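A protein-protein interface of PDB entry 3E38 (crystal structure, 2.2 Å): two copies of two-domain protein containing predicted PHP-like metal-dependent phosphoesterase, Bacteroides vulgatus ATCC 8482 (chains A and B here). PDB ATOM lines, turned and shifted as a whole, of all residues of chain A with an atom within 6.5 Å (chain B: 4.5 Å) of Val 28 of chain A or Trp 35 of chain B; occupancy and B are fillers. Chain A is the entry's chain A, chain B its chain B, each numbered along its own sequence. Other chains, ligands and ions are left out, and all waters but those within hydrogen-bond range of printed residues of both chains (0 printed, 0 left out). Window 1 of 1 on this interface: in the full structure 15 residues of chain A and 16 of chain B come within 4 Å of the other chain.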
ATOM      1  N   HIS A  26     -16.303  19.355  28.997  1.00  0.00           N
ATOM      2  CA  HIS A  26     -16.347  19.746  27.584  1.00  0.00           C
ATOM      3  C   HIS A  26     -16.950  18.742  26.640  1.00  0.00           C
ATOM      4  O   HIS A  26     -17.037  17.562  26.925  1.00  0.00           O
ATOM      5  CB  HIS A  26     -14.925  20.093  27.109  1.00  0.00           C
ATOM      6  CG  HIS A  26     -14.261  21.131  27.936  1.00  0.00           C
ATOM      7  ND1 HIS A  26     -14.278  22.471  27.615  1.00  0.00           N
ATOM      8  CD2 HIS A  26     -13.562  21.027  29.090  1.00  0.00           C
ATOM      9  CE1 HIS A  26     -13.619  23.149  28.543  1.00  0.00           C
ATOM     10  NE2 HIS A  26     -13.166  22.289  29.447  1.00  0.00           N
ATOM     11  N   SER A  27     -17.399  19.271  25.506  1.00  0.00           N
ATOM     12  CA  SER A  27     -17.972  18.459  24.421  1.00  0.00           C
ATOM     13  C   SER A  27     -17.383  18.945  23.125  1.00  0.00           C
ATOM     14  O   SER A  27     -16.527  19.823  23.128  1.00  0.00           O
ATOM     15  CB  SER A  27     -19.478  18.596  24.309  1.00  0.00           C
ATOM     16  OG  SER A  27     -19.894  19.906  23.845  1.00  0.00           O
ATOM     17  N   VAL A  28     -17.945  18.432  22.037  1.00  0.00           N
ATOM     18  CA  VAL A  28     -17.507  18.742  20.694  1.00  0.00           C
ATOM     19  C   VAL A  28     -17.713  20.207  20.332  1.00  0.00           C
ATOM     20  O   VAL A  28     -17.154  20.669  19.354  1.00  0.00           O
ATOM     21  CB  VAL A  28     -18.185  17.810  19.555  1.00  0.00           C
ATOM     22  CG1 VAL A  28     -17.708  16.355  19.669  1.00  0.00           C
ATOM     23  CG2 VAL A  28     -19.674  17.906  19.547  1.00  0.00           C
ATOM     24  N   PHE A  29     -18.474  20.908  21.156  1.00  0.00           N
ATOM     25  CA  PHE A  29     -18.891  22.309  20.934  1.00  0.00           C
ATOM     26  C   PHE A  29     -17.765  23.227  21.364  1.00  0.00           C
ATOM     27  O   PHE A  29     -17.798  24.445  21.140  1.00  0.00           O
ATOM     28  CB  PHE A  29     -20.240  22.634  21.555  1.00  0.00           C
ATOM     29  CG  PHE A  29     -21.398  22.160  20.692  1.00  0.00           C
ATOM     30  CD1 PHE A  29     -21.831  20.856  20.752  1.00  0.00           C
ATOM     31  CD2 PHE A  29     -21.955  22.991  19.748  1.00  0.00           C
ATOM     32  CE1 PHE A  29     -22.802  20.405  19.915  1.00  0.00           C
ATOM     33  CE2 PHE A  29     -22.948  22.538  18.915  1.00  0.00           C
ATOM     34  CZ  PHE A  29     -23.382  21.246  19.028  1.00  0.00           C
ATOM     35  N   SER A  30     -16.765  22.620  22.008  1.00  0.00           N
ATOM     36  CA  SER A  30     -15.449  23.277  22.274  1.00  0.00           C
ATOM     37  C   SER A  30     -14.370  22.265  21.859  1.00  0.00           C
ATOM     38  O   SER A  30     -14.310  21.861  20.682  1.00  0.00           O
ATOM     39  CB  SER A  30     -15.256  23.834  23.703  1.00  0.00           C
ATOM     40  OG  SER A  30     -15.402  22.883  24.750  1.00  0.00           O
ATOM     41  N   ASP A  31     -13.552  21.827  22.814  1.00  0.00           N
ATOM     42  CA  ASP A  31     -12.489  20.847  22.516  1.00  0.00           C
ATOM     43  C   ASP A  31     -12.715  19.485  23.127  1.00  0.00           C
ATOM     44  O   ASP A  31     -11.818  18.680  23.177  1.00  0.00           O
ATOM     45  CB  ASP A  31     -11.095  21.326  22.909  1.00  0.00           C
ATOM     46  CG  ASP A  31     -10.937  21.481  24.397  1.00  0.00           C
ATOM     47  OD1 ASP A  31     -11.940  21.424  25.126  1.00  0.00           O
ATOM     48  OD2 ASP A  31      -9.797  21.687  24.827  1.00  0.00           O
ATOM     49  N   GLY A  32     -13.926  19.226  23.575  1.00  0.00           N
ATOM     50  CA  GLY A  32     -14.289  17.894  24.045  1.00  0.00           C
ATOM     51  C   GLY A  32     -14.515  16.969  22.872  1.00  0.00           C
ATOM     52  O   GLY A  32     -14.533  17.395  21.719  1.00  0.00           O
ATOM     53  N   LEU A  33     -14.810  15.714  23.173  1.00  0.00           N
ATOM     54  CA  LEU A  33     -14.825  14.673  22.151  1.00  0.00           C
ATOM     55  C   LEU A  33     -16.097  13.860  22.061  1.00  0.00           C
ATOM     56  O   LEU A  33     -16.175  12.866  21.305  1.00  0.00           O
ATOM     57  CB  LEU A  33     -13.623  13.738  22.372  1.00  0.00           C
ATOM     58  CG  LEU A  33     -12.276  14.410  22.032  1.00  0.00           C
ATOM     59  CD1 LEU A  33     -11.134  13.527  22.380  1.00  0.00           C
ATOM     60  CD2 LEU A  33     -12.146  14.776  20.545  1.00  0.00           C
ATOM     61  N   VAL A  34     -17.096  14.331  22.807  1.00  0.00           N
ATOM     62  CA  VAL A  34     -18.423  13.700  22.822  1.00  0.00           C
ATOM     63  C   VAL A  34     -19.521  14.686  22.576  1.00  0.00           C
ATOM     64  O   VAL A  34     -19.409  15.895  22.848  1.00  0.00           O
ATOM     65  CB  VAL A  34     -18.743  13.010  24.177  1.00  0.00           C
ATOM     66  CG1 VAL A  34     -17.682  11.948  24.511  1.00  0.00           C
ATOM     67  CG2 VAL A  34     -18.857  14.038  25.304  1.00  0.00           C
ATOM     68  N   TRP A  35     -20.597  14.146  22.029  1.00  0.00           N
ATOM     69  CA  TRP A  35     -21.815  14.927  21.827  1.00  0.00           C
ATOM     70  C   TRP A  35     -22.326  15.347  23.223  1.00  0.00           C
ATOM     71  O   TRP A  35     -22.218  14.594  24.233  1.00  0.00           O
ATOM     72  CB  TRP A  35     -22.855  14.114  21.004  1.00  0.00           C
ATOM     73  CG  TRP A  35     -24.016  14.937  20.488  1.00  0.00           C
ATOM     74  CD1 TRP A  35     -25.311  14.854  20.886  1.00  0.00           C
ATOM     75  CD2 TRP A  35     -23.971  15.969  19.480  1.00  0.00           C
ATOM     76  NE1 TRP A  35     -26.075  15.760  20.201  1.00  0.00           N
ATOM     77  CE2 TRP A  35     -25.277  16.459  19.333  1.00  0.00           C
ATOM     78  CE3 TRP A  35     -22.955  16.510  18.685  1.00  0.00           C
ATOM     79  CZ2 TRP A  35     -25.600  17.469  18.426  1.00  0.00           C
ATOM     80  CZ3 TRP A  35     -23.268  17.531  17.793  1.00  0.00           C
ATOM     81  CH2 TRP A  35     -24.587  17.996  17.673  1.00  0.00           C
ATOM     82  N   PRO A  36     -22.890  16.548  23.322  1.00  0.00           N
ATOM     83  CA  PRO A  36     -23.255  17.006  24.678  1.00  0.00           C
ATOM     84  C   PRO A  36     -24.180  16.094  25.469  1.00  0.00           C
ATOM     85  O   PRO A  36     -24.049  15.984  26.668  1.00  0.00           O
ATOM     86  CB  PRO A  36     -23.933  18.340  24.416  1.00  0.00           C
ATOM     87  CG  PRO A  36     -23.463  18.764  23.079  1.00  0.00           C
ATOM     88  CD  PRO A  36     -23.125  17.567  22.291  1.00  0.00           C
ATOM     89  N   GLU A  55     -18.070  24.891  27.924  1.00  0.00           N
ATOM     90  CA  GLU A  55     -17.281  24.936  26.716  1.00  0.00           C
ATOM     91  C   GLU A  55     -16.309  26.154  26.792  1.00  0.00           C
ATOM     92  O   GLU A  55     -16.609  27.179  27.384  1.00  0.00           O
ATOM     93  CB  GLU A  55     -18.144  25.075  25.469  1.00  0.00           C
ATOM     94  CG  GLU A  55     -19.370  24.166  25.293  1.00  0.00           C
ATOM     95  CD  GLU A  55     -19.113  22.658  25.306  1.00  0.00           C
ATOM     96  OE1 GLU A  55     -17.953  22.192  25.308  1.00  0.00           O
ATOM     97  OE2 GLU A  55     -20.130  21.944  25.269  1.00  0.00           O
ATOM     98  N   ARG A  60     -12.397  26.839  20.242  1.00  0.00           N
ATOM     99  CA  ARG A  60     -13.349  25.920  19.615  1.00  0.00           C
ATOM    100  C   ARG A  60     -12.698  25.372  18.341  1.00  0.00           C
ATOM    101  O   ARG A  60     -12.905  25.900  17.266  1.00  0.00           O
ATOM    102  CB  ARG A  60     -14.657  26.649  19.312  1.00  0.00           C
ATOM    103  CG  ARG A  60     -15.289  27.199  20.547  1.00  0.00           C
ATOM    104  CD  ARG A  60     -16.598  27.828  20.251  1.00  0.00           C
ATOM    105  NE  ARG A  60     -16.441  29.043  19.476  1.00  0.00           N
ATOM    106  CZ  ARG A  60     -17.457  29.741  18.983  1.00  0.00           C
ATOM    107  NH1 ARG A  60     -18.713  29.320  19.138  1.00  0.00           N
ATOM    108  NH2 ARG A  60     -17.210  30.848  18.309  1.00  0.00           N
ATOM    109  N   PRO A  61     -11.861  24.341  18.474  1.00  0.00           N
ATOM    110  CA  PRO A  61     -11.112  23.837  17.347  1.00  0.00           C
ATOM    111  C   PRO A  61     -11.933  23.042  16.356  1.00  0.00           C
ATOM    112  O   PRO A  61     -11.442  22.706  15.287  1.00  0.00           O
ATOM    113  CB  PRO A  61     -10.043  22.952  17.997  1.00  0.00           C
ATOM    114  CG  PRO A  61     -10.525  22.631  19.327  1.00  0.00           C
ATOM    115  CD  PRO A  61     -11.523  23.646  19.725  1.00  0.00           C
ATOM    116  N   HIS A  62     -13.188  22.787  16.672  1.00  0.00           N
ATOM    117  CA  HIS A  62     -14.025  22.072  15.709  1.00  0.00           C
ATOM    118  C   HIS A  62     -14.954  23.046  15.008  1.00  0.00           C
ATOM    119  O   HIS A  62     -15.796  22.646  14.236  1.00  0.00           O
ATOM    120  CB  HIS A  62     -14.865  21.010  16.415  1.00  0.00           C
ATOM    121  CG  HIS A  62     -14.056  20.030  17.207  1.00  0.00           C
ATOM    122  ND1 HIS A  62     -14.388  19.660  18.485  1.00  0.00           N
ATOM    123  CD2 HIS A  62     -12.919  19.361  16.906  1.00  0.00           C
ATOM    124  CE1 HIS A  62     -13.499  18.794  18.932  1.00  0.00           C
ATOM    125  NE2 HIS A  62     -12.602  18.590  17.989  1.00  0.00           N
ATOM    126  N   LYS A  63     -14.801  24.338  15.251  1.00  0.00           N
ATOM    127  CA  LYS A  63     -15.844  25.265  14.745  1.00  0.00           C
ATOM    128  C   LYS A  63     -16.112  25.315  13.256  1.00  0.00           C
ATOM    129  O   LYS A  63     -17.128  25.862  12.817  1.00  0.00           O
ATOM    130  CB  LYS A  63     -15.622  26.691  15.256  1.00  0.00           C
ATOM    131  CG  LYS A  63     -14.431  27.397  14.801  1.00  0.00           C
ATOM    132  CD  LYS A  63     -14.613  28.807  15.296  1.00  0.00           C
ATOM    133  CE  LYS A  63     -13.338  29.587  15.292  1.00  0.00           C
ATOM    134  NZ  LYS A  63     -13.608  30.994  15.733  1.00  0.00           N
ATOM    135  N   ASP A  65     -16.671  22.796  11.536  1.00  0.00           N
ATOM    136  CA  ASP A  65     -17.670  21.725  11.408  1.00  0.00           C
ATOM    137  C   ASP A  65     -18.819  21.932  12.374  1.00  0.00           C
ATOM    138  O   ASP A  65     -19.952  21.698  12.017  1.00  0.00           O
ATOM    139  CB  ASP A  65     -17.075  20.339  11.720  1.00  0.00           C
ATOM    140  CG  ASP A  65     -16.019  19.921  10.733  1.00  0.00           C
ATOM    141  OD1 ASP A  65     -16.314  19.872   9.514  1.00  0.00           O
ATOM    142  OD2 ASP A  65     -14.892  19.631  11.187  1.00  0.00           O
ATOM    143  N   VAL A  66     -18.497  22.382  13.594  1.00  0.00           N
ATOM    144  CA  VAL A  66     -19.492  22.581  14.697  1.00  0.00           C
ATOM    145  C   VAL A  66     -19.692  24.067  14.747  1.00  0.00           C
ATOM    146  O   VAL A  66     -19.045  24.811  15.486  1.00  0.00           O
ATOM    147  CB  VAL A  66     -19.007  21.941  16.024  1.00  0.00           C
ATOM    148  CG1 VAL A  66     -20.116  21.947  17.021  1.00  0.00           C
ATOM    149  CG2 VAL A  66     -18.514  20.486  15.754  1.00  0.00           C
ATOM    150  N   SER B  27     -20.277   8.334  13.921  1.00  0.00           N
ATOM    151  CA  SER B  27     -19.776   9.509  14.650  1.00  0.00           C
ATOM    152  C   SER B  27     -20.868  10.575  14.641  1.00  0.00           C
ATOM    153  O   SER B  27     -21.945  10.358  14.140  1.00  0.00           O
ATOM    154  CB  SER B  27     -18.481  10.078  14.066  1.00  0.00           C
ATOM    155  OG  SER B  27     -18.664  10.859  12.871  1.00  0.00           O
ATOM    156  N   VAL B  28     -20.573  11.712  15.236  1.00  0.00           N
ATOM    157  CA  VAL B  28     -21.523  12.806  15.310  1.00  0.00           C
ATOM    158  C   VAL B  28     -21.874  13.406  13.918  1.00  0.00           C
ATOM    159  O   VAL B  28     -22.703  14.322  13.809  1.00  0.00           O
ATOM    160  CB  VAL B  28     -20.953  13.983  16.214  1.00  0.00           C
ATOM    161  CG1 VAL B  28     -20.956  13.595  17.689  1.00  0.00           C
ATOM    162  CG2 VAL B  28     -19.596  14.415  15.740  1.00  0.00           C
ATOM    163  N   PHE B  29     -21.212  12.879  12.883  1.00  0.00           N
ATOM    164  CA  PHE B  29     -21.356  13.351  11.498  1.00  0.00           C
ATOM    165  C   PHE B  29     -22.545  12.635  10.869  1.00  0.00           C
ATOM    166  O   PHE B  29     -22.972  12.939   9.771  1.00  0.00           O
ATOM    167  CB  PHE B  29     -20.040  13.280  10.722  1.00  0.00           C
ATOM    168  CG  PHE B  29     -19.095  14.440  11.032  1.00  0.00           C
ATOM    169  CD1 PHE B  29     -18.267  14.419  12.129  1.00  0.00           C
ATOM    170  CD2 PHE B  29     -19.022  15.526  10.205  1.00  0.00           C
ATOM    171  CE1 PHE B  29     -17.445  15.485  12.428  1.00  0.00           C
ATOM    172  CE2 PHE B  29     -18.213  16.612  10.494  1.00  0.00           C
ATOM    173  CZ  PHE B  29     -17.398  16.571  11.610  1.00  0.00           C
ATOM    174  N   VAL B  34     -19.839  10.413  19.215  1.00  0.00           N
ATOM    175  CA  VAL B  34     -18.432  10.791  19.422  1.00  0.00           C
ATOM    176  C   VAL B  34     -17.818  11.488  18.214  1.00  0.00           C
ATOM    177  O   VAL B  34     -18.246  11.314  17.055  1.00  0.00           O
ATOM    178  CB  VAL B  34     -17.569   9.549  19.770  1.00  0.00           C
ATOM    179  CG1 VAL B  34     -18.048   8.941  21.099  1.00  0.00           C
ATOM    180  CG2 VAL B  34     -17.550   8.467  18.614  1.00  0.00           C
ATOM    181  N   TRP B  35     -16.806  12.286  18.501  1.00  0.00           N
ATOM    182  CA  TRP B  35     -16.000  12.910  17.452  1.00  0.00           C
ATOM    183  C   TRP B  35     -15.266  11.805  16.648  1.00  0.00           C
ATOM    184  O   TRP B  35     -14.851  10.807  17.222  1.00  0.00           O
ATOM    185  CB  TRP B  35     -15.018  13.889  18.063  1.00  0.00           C
ATOM    186  CG  TRP B  35     -14.363  14.686  17.054  1.00  0.00           C
ATOM    187  CD1 TRP B  35     -13.102  14.569  16.652  1.00  0.00           C
ATOM    188  CD2 TRP B  35     -14.932  15.780  16.314  1.00  0.00           C
ATOM    189  NE1 TRP B  35     -12.824  15.503  15.687  1.00  0.00           N
ATOM    190  CE2 TRP B  35     -13.932  16.261  15.459  1.00  0.00           C
ATOM    191  CE3 TRP B  35     -16.202  16.377  16.270  1.00  0.00           C
ATOM    192  CZ2 TRP B  35     -14.132  17.346  14.583  1.00  0.00           C
ATOM    193  CZ3 TRP B  35     -16.409  17.445  15.366  1.00  0.00           C
ATOM    194  CH2 TRP B  35     -15.375  17.911  14.552  1.00  0.00           C
ATOM    195  N   PRO B  36     -15.083  11.983  15.323  1.00  0.00           N
ATOM    196  CA  PRO B  36     -14.603  10.791  14.575  1.00  0.00           C
ATOM    197  C   PRO B  36     -13.298  10.215  15.019  1.00  0.00           C
ATOM    198  O   PRO B  36     -13.142   9.019  14.910  1.00  0.00           O
ATOM    199  CB  PRO B  36     -14.512  11.303  13.139  1.00  0.00           C
ATOM    200  CG  PRO B  36     -15.621  12.327  13.086  1.00  0.00           C
ATOM    201  CD  PRO B  36     -15.435  13.081  14.391  1.00  0.00           C
ATOM    202  N   THR B  37     -12.414  11.027  15.608  1.00  0.00           N
ATOM    203  CA  THR B  37     -11.085  10.530  15.967  1.00  0.00           C
ATOM    204  C   THR B  37     -11.177   9.520  17.128  1.00  0.00           C
ATOM    205  O   THR B  37     -10.365   8.616  17.299  1.00  0.00           O
ATOM    206  CB  THR B  37     -10.137  11.655  16.227  1.00  0.00           C
ATOM    207  OG1 THR B  37     -10.691  12.520  17.208  1.00  0.00           O
ATOM    208  CG2 THR B  37      -9.947  12.429  14.904  1.00  0.00           C
ATOM    209  N   VAL B  38     -12.254   9.608  17.862  1.00  0.00           N
ATOM    210  CA  VAL B  38     -12.446   8.674  18.953  1.00  0.00           C
ATOM    211  C   VAL B  38     -12.563   7.266  18.401  1.00  0.00           C
ATOM    212  O   VAL B  38     -12.131   6.317  19.048  1.00  0.00           O
ATOM    213  CB  VAL B  38     -13.731   8.999  19.742  1.00  0.00           C
ATOM    214  CG1 VAL B  38     -14.007   7.967  20.815  1.00  0.00           C
ATOM    215  CG2 VAL B  38     -13.631  10.354  20.323  1.00  0.00           C
ATOM    216  N   ARG B  39     -13.159   7.117  17.219  1.00  0.00           N
ATOM    217  CA  ARG B  39     -13.340   5.761  16.699  1.00  0.00           C
ATOM    218  C   ARG B  39     -11.988   5.120  16.389  1.00  0.00           C
ATOM    219  O   ARG B  39     -11.854   3.884  16.370  1.00  0.00           O
ATOM    220  CB  ARG B  39     -14.226   5.692  15.446  1.00  0.00           C
ATOM    221  CG  ARG B  39     -15.691   6.060  15.639  1.00  0.00           C
ATOM    222  CD  ARG B  39     -16.318   5.244  16.742  1.00  0.00           C
ATOM    223  NE  ARG B  39     -17.731   5.566  16.911  1.00  0.00           N
ATOM    224  CZ  ARG B  39     -18.410   5.413  18.048  1.00  0.00           C
ATOM    225  NH1 ARG B  39     -17.808   4.946  19.141  1.00  0.00           N
ATOM    226  NH2 ARG B  39     -19.697   5.728  18.091  1.00  0.00           N
ATOM    227  N   LEU B  76     -11.395  13.407   8.606  1.00  0.00           N
ATOM    228  CA  LEU B  76     -10.910  13.778   9.966  1.00  0.00           C
ATOM    229  C   LEU B  76     -10.145  12.675  10.691  1.00  0.00           C
ATOM    230  O   LEU B  76      -9.407  12.919  11.637  1.00  0.00           O
ATOM    231  CB  LEU B  76     -12.099  14.190  10.848  1.00  0.00           C
ATOM    232  CG  LEU B  76     -12.710  15.542  10.509  1.00  0.00           C
ATOM    233  CD1 LEU B  76     -14.054  15.731  11.155  1.00  0.00           C
ATOM    234  CD2 LEU B  76     -11.707  16.662  10.945  1.00  0.00           C
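Of the 18 printed residues of chain A, 6 touch a printed residue of chain B.
Printed residues of chain A that touch a printed residue of chain B: Val 28, Leu 33, Trp 35, His 62, Asp 65 and Val 66.
Hydrophobic or aromatic side chains of chain A within 4 Å of the printed part of chain B: Val 28, Leu 33, Trp 35, His 62 and Val 66.
Of the 10 printed residues of chain B, 6 touch a printed residue of chain A.
Hydrophobic or aromatic side chains of chain B within 4 Å of the printed part of chain A: Val 28, Phe 29, Val 34, Trp 35, Val 38 and Leu 76.
Among the printed residues, no Asp or Glu carboxylate lies within 4 Å of a Lys or Arg side-chain nitrogen of the other chain.
The backbone NH (N) of Val 28 of chain A sits at hydrogen-bond distance from the backbone carbonyl oxygen (O) of Val 34 of chain A, at 3.0 Å.
The backbone carbonyl oxygen (O) of Val 28 of chain A sits at hydrogen-bond distance from a ring nitrogen (ND1) of His 62 of chain A (3.1 Å).
The backbone carbonyl oxygen of Ser 30 of chain A is in hydrogen-bond range of a ring nitrogen (ND1) of His 62 of chain A.
The side-chain hydroxyl of Ser 27 of chain B sits close to the backbone NH of Phe 29 of chain B (3.3 Å).
The backbone NH (N) of Val 28 of chain B sits at hydrogen-bond distance from the backbone carbonyl oxygen (O) of Val 34 of chain B, at 3.0 Å.
Val 28 of chain A touches Trp 35 of chain B, and with the chains exchanged Trp 35 of chain A touches Val 28 of chain B.
6 positions are printed for both chains.
Of the 10 pairs that touch across the chains among the printed residues, 2 have their exchanged pair printed and touching as well.
Among the printed residues, pairs that only touch across the chains: Val 28 of chain A with Trp 35 of chain B, Leu 33 of chain A with Val 34 of chain B, Leu 33 of chain A with Val 38 of chain B, Trp 35 of chain A with Val 28 of chain B, His 62 of chain A with Trp 35 of chain B, Asp 65 of chain A with Phe 29 of chain B, Asp 65 of chain A with Trp 35 of chain B, Asp 65 of chain A with Leu 76 of chain B and Val 66 of chain A with Trp 35 of chain B.
O of Leu 33 of chain A is in hydrogen-bond range of N of Trp 35 of chain B (2.9 Å).
Printed residues of chain B within 4 Å of Val 28 of chain A: Trp 35 (3.7 Å).
Of chain A, only Val 28, Leu 33, His 62, Asp 65 and Val 66 come within 4 Å of Trp 35 of chain B.
Printed residues of chain A within 4 Å of Leu 76 of chain B: Asp 65.
Printed residues of chain B within 4 Å of His 62 of chain A: Trp 35 (3.3 Å).
Printed residues of chain B within 4 Å of Trp 35 of chain A: Val 28.
Pro 36 of chain A touches none of the printed residues of chain B.
Ser 27 of chain A touches none of the printed residues of chain B.
The nearest printed residue of chain B that does not touch Val 28 of chain A is Val 28 of chain B (4.7 Å).
The nearest printed residue of chain A that does not touch Val 38 of chain B is Val 34 of chain A (5.8 Å).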
